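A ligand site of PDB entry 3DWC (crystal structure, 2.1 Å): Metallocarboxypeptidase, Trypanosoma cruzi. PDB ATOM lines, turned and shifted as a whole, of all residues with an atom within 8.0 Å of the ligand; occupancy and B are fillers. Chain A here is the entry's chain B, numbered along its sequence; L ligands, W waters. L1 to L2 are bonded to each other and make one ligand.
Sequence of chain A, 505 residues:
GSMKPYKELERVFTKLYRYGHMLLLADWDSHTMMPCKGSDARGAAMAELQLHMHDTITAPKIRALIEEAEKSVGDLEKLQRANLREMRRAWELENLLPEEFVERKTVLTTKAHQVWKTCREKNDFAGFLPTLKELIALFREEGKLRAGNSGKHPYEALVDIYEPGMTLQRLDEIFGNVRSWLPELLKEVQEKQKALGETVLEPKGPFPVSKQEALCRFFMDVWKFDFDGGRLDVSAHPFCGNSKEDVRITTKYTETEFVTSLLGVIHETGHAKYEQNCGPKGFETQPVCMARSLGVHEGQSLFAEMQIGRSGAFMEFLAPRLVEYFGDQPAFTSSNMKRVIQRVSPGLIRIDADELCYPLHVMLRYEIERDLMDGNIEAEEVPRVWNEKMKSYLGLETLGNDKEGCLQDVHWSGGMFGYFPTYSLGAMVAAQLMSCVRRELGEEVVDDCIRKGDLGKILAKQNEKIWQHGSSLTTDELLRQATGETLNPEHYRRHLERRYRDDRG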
ATOM      1  N   ASP A 221      -0.412  -6.496  34.192  1.00  0.00           N
ATOM      2  CA  ASP A 221      -0.079  -7.946  34.096  1.00  0.00           C
ATOM      3  C   ASP A 221       0.004  -8.488  32.662  1.00  0.00           C
ATOM      4  O   ASP A 221       0.876  -9.318  32.325  1.00  0.00           O
ATOM      5  CB  ASP A 221      -1.112  -8.788  34.872  1.00  0.00           C
ATOM      6  CG  ASP A 221      -0.976  -8.662  36.383  1.00  0.00           C
ATOM      7  OD1 ASP A 221       0.077  -8.185  36.893  1.00  0.00           O
ATOM      8  OD2 ASP A 221      -1.949  -9.062  37.075  1.00  0.00           O
ATOM      9  N   VAL A 222      -0.888  -8.024  31.792  1.00  0.00           N
ATOM     10  CA  VAL A 222      -0.848  -8.357  30.369  1.00  0.00           C
ATOM     11  C   VAL A 222       0.487  -7.909  29.783  1.00  0.00           C
ATOM     12  O   VAL A 222       1.066  -8.623  28.993  1.00  0.00           O
ATOM     13  CB  VAL A 222      -2.061  -7.753  29.590  1.00  0.00           C
ATOM     14  CG1 VAL A 222      -1.898  -7.877  28.080  1.00  0.00           C
ATOM     15  CG2 VAL A 222      -3.400  -8.380  30.103  1.00  0.00           C
ATOM     16  N   LYS A 224       3.210  -7.826  31.414  1.00  0.00           N
ATOM     17  CA  LYS A 224       4.180  -8.512  32.259  1.00  0.00           C
ATOM     18  C   LYS A 224       5.013  -7.544  33.085  1.00  0.00           C
ATOM     19  O   LYS A 224       6.168  -7.777  33.367  1.00  0.00           O
ATOM     20  CB  LYS A 224       4.997  -9.484  31.419  1.00  0.00           C
ATOM     21  CG  LYS A 224       4.079 -10.285  30.519  1.00  0.00           C
ATOM     22  CD  LYS A 224       4.734 -11.425  29.878  1.00  0.00           C
ATOM     23  CE  LYS A 224       3.821 -12.037  28.788  1.00  0.00           C
ATOM     24  NZ  LYS A 224       2.560 -12.797  29.280  1.00  0.00           N
ATOM     25  N   CYS A 449      -1.401 -12.363  18.900  1.00  0.00           N
ATOM     26  CA  CYS A 449      -0.851 -11.948  20.189  1.00  0.00           C
ATOM     27  C   CYS A 449      -1.648 -10.829  20.830  1.00  0.00           C
ATOM     28  O   CYS A 449      -1.980 -10.882  22.010  1.00  0.00           O
ATOM     29  CB  CYS A 449       0.610 -11.504  20.057  1.00  0.00           C
ATOM     30  SG  CYS A 449       1.771 -12.817  19.528  1.00  0.00           S
ATOM     31  N   LYS A 452      -5.511 -11.811  21.665  1.00  0.00           N
ATOM     32  CA  LYS A 452      -5.548 -12.730  22.775  1.00  0.00           C
ATOM     33  C   LYS A 452      -4.823 -12.212  24.041  1.00  0.00           C
ATOM     34  O   LYS A 452      -4.768 -12.932  25.035  1.00  0.00           O
ATOM     35  CB  LYS A 452      -4.899 -14.074  22.381  1.00  0.00           C
ATOM     36  CG  LYS A 452      -5.588 -14.816  21.245  1.00  0.00           C
ATOM     37  CD  LYS A 452      -4.880 -16.152  20.985  1.00  0.00           C
ATOM     38  CE  LYS A 452      -5.467 -16.898  19.750  1.00  0.00           C
ATOM     39  NZ  LYS A 452      -4.755 -18.185  19.498  1.00  0.00           N
ATOM     40  N   GLY A 453      -4.245 -11.011  24.017  1.00  0.00           N
ATOM     41  CA  GLY A 453      -3.568 -10.493  25.198  1.00  0.00           C
ATOM     42  C   GLY A 453      -2.374 -11.341  25.640  1.00  0.00           C
ATOM     43  O   GLY A 453      -2.108 -11.487  26.830  1.00  0.00           O
ATOM     44  N   ASP A 454      -1.681 -11.877  24.636  1.00  0.00           N
ATOM     45  CA  ASP A 454      -0.521 -12.749  24.750  1.00  0.00           C
ATOM     46  C   ASP A 454       0.689 -12.046  24.137  1.00  0.00           C
ATOM     47  O   ASP A 454       1.137 -12.364  23.019  1.00  0.00           O
ATOM     48  CB  ASP A 454      -0.837 -14.025  23.952  1.00  0.00           C
ATOM     49  CG  ASP A 454       0.015 -15.177  24.333  1.00  0.00           C
ATOM     50  OD1 ASP A 454       0.752 -15.039  25.324  1.00  0.00           O
ATOM     51  OD2 ASP A 454      -0.052 -16.244  23.620  1.00  0.00           O
ATOM     52  N   LEU A 455       1.250 -11.103  24.887  1.00  0.00           N
ATOM     53  CA  LEU A 455       2.245 -10.180  24.315  1.00  0.00           C
ATOM     54  C   LEU A 455       3.695 -10.593  24.370  1.00  0.00           C
ATOM     55  O   LEU A 455       4.528  -9.932  23.795  1.00  0.00           O
ATOM     56  CB  LEU A 455       2.113  -8.788  24.915  1.00  0.00           C
ATOM     57  CG  LEU A 455       0.733  -8.138  24.784  1.00  0.00           C
ATOM     58  CD1 LEU A 455       0.761  -6.830  25.571  1.00  0.00           C
ATOM     59  CD2 LEU A 455       0.295  -7.914  23.335  1.00  0.00           C
ATOM     60  N   GLY A 456       4.006 -11.709  24.990  1.00  0.00           N
ATOM     61  CA  GLY A 456       5.402 -12.084  25.240  1.00  0.00           C
ATOM     62  C   GLY A 456       6.322 -12.075  24.025  1.00  0.00           C
ATOM     63  O   GLY A 456       7.497 -11.740  24.142  1.00  0.00           O
ATOM     64  N   LYS A 457       5.812 -12.460  22.854  1.00  0.00           N
ATOM     65  CA  LYS A 457       6.663 -12.554  21.645  1.00  0.00           C
ATOM     66  C   LYS A 457       6.998 -11.138  21.174  1.00  0.00           C
ATOM     67  O   LYS A 457       8.114 -10.808  20.655  1.00  0.00           O
ATOM     68  CB  LYS A 457       5.939 -13.308  20.553  1.00  0.00           C
ATOM     69  CG  LYS A 457       6.036 -14.809  20.650  1.00  0.00           C
ATOM     70  CD  LYS A 457       5.144 -15.441  19.619  1.00  0.00           C
ATOM     71  CE  LYS A 457       5.220 -16.943  19.705  1.00  0.00           C
ATOM     72  NZ  LYS A 457       4.654 -17.542  18.449  1.00  0.00           N
ATOM     73  N   ILE A 458       6.014 -10.257  21.377  1.00  0.00           N
ATOM     74  CA  ILE A 458       6.186  -8.875  20.992  1.00  0.00           C
ATOM     75  C   ILE A 458       7.159  -8.243  21.963  1.00  0.00           C
ATOM     76  O   ILE A 458       8.129  -7.640  21.536  1.00  0.00           O
ATOM     77  CB  ILE A 458       4.857  -8.122  20.916  1.00  0.00           C
ATOM     78  CG1 ILE A 458       3.886  -8.766  19.906  1.00  0.00           C
ATOM     79  CG2 ILE A 458       5.079  -6.653  20.466  1.00  0.00           C
ATOM     80  CD1 ILE A 458       2.463  -8.079  19.981  1.00  0.00           C
ATOM     81  N   LEU A 459       6.931  -8.416  23.276  1.00  0.00           N
ATOM     82  CA  LEU A 459       7.748  -7.784  24.293  1.00  0.00           C
ATOM     83  C   LEU A 459       9.179  -8.294  24.167  1.00  0.00           C
ATOM     84  O   LEU A 459      10.105  -7.522  24.346  1.00  0.00           O
ATOM     85  CB  LEU A 459       7.202  -8.028  25.728  1.00  0.00           C
ATOM     86  CG  LEU A 459       5.760  -7.579  25.996  1.00  0.00           C
ATOM     87  CD1 LEU A 459       5.271  -8.085  27.343  1.00  0.00           C
ATOM     88  CD2 LEU A 459       5.665  -6.031  25.865  1.00  0.00           C
ATOM     89  N   ALA A 460       9.368  -9.567  23.806  1.00  0.00           N
ATOM     90  CA  ALA A 460      10.703 -10.113  23.645  1.00  0.00           C
ATOM     91  C   ALA A 460      11.487  -9.439  22.522  1.00  0.00           C
ATOM     92  O   ALA A 460      12.680  -9.181  22.653  1.00  0.00           O
ATOM     93  CB  ALA A 460      10.675 -11.618  23.415  1.00  0.00           C
ATOM     94  N   LYS A 461      10.824  -9.149  21.420  1.00  0.00           N
ATOM     95  CA  LYS A 461      11.461  -8.392  20.309  1.00  0.00           C
ATOM     96  C   LYS A 461      11.857  -6.987  20.739  1.00  0.00           C
ATOM     97  O   LYS A 461      12.916  -6.506  20.351  1.00  0.00           O
ATOM     98  CB  LYS A 461      10.505  -8.250  19.123  1.00  0.00           C
ATOM     99  CG  LYS A 461      10.289  -9.453  18.297  1.00  0.00           C
ATOM    100  CD  LYS A 461      11.515  -9.766  17.396  1.00  0.00           C
ATOM    101  CE  LYS A 461      11.344 -11.133  16.703  1.00  0.00           C
ATOM    102  NZ  LYS A 461      12.485 -11.422  15.771  1.00  0.00           N
HETATM  103  N1  LIG L   1       2.742 -13.783  26.385  1.00  0.00           N
HETATM  104  C1  LIG L   1       3.216 -15.064  26.955  1.00  0.00           C
HETATM  105  C2  LIG L   1       4.670 -15.426  26.704  1.00  0.00           C
HETATM  106  O1  LIG L   1       5.499 -15.404  27.639  1.00  0.00           O
HETATM  107  N1  LG2 L   2       4.967 -15.704  25.432  1.00  0.00           N
HETATM  108  C1  LG2 L   2       6.237 -16.327  24.988  1.00  0.00           C
HETATM  109  C2  LG2 L   2       7.406 -15.346  24.970  1.00  0.00           C
HETATM  110  O1  LG2 L   2       8.213 -15.327  24.039  1.00  0.00           O
HETATM  111  C3  LG2 L   2       6.037 -16.962  23.601  1.00  0.00           C
HETATM  112  O   HOH W   1       9.886 -15.351  22.082  1.00  0.00           O
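OD1 of Asp 454 is in salt-bridge range of N1 of LIG L1 (2.6 Å).
The backbone NH (N) of Leu 455 lies close to a nitrogen (N1) of LIG L1 (3.4 Å).
The side-chain amino group (NZ) of Lys 224 lies close to a nitrogen (N1) of LIG L1, at 3.1 Å.
N1 of LIG L1 sits close to N of Gly 456 (2.8 Å).
N of Asp 454 sits at hydrogen-bond distance from O of Cys 449, at 2.8 Å.
Merely in contact with the ligand: Lys 457.
Of the 14 residues printed, 5 come within 4 Å of the ligand.
Along chain A the residues within 4 Å of the ligand span positions 224 to 457.
The nearest printed residue that does not touch the ligand is Ala 460 (4.5 Å).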
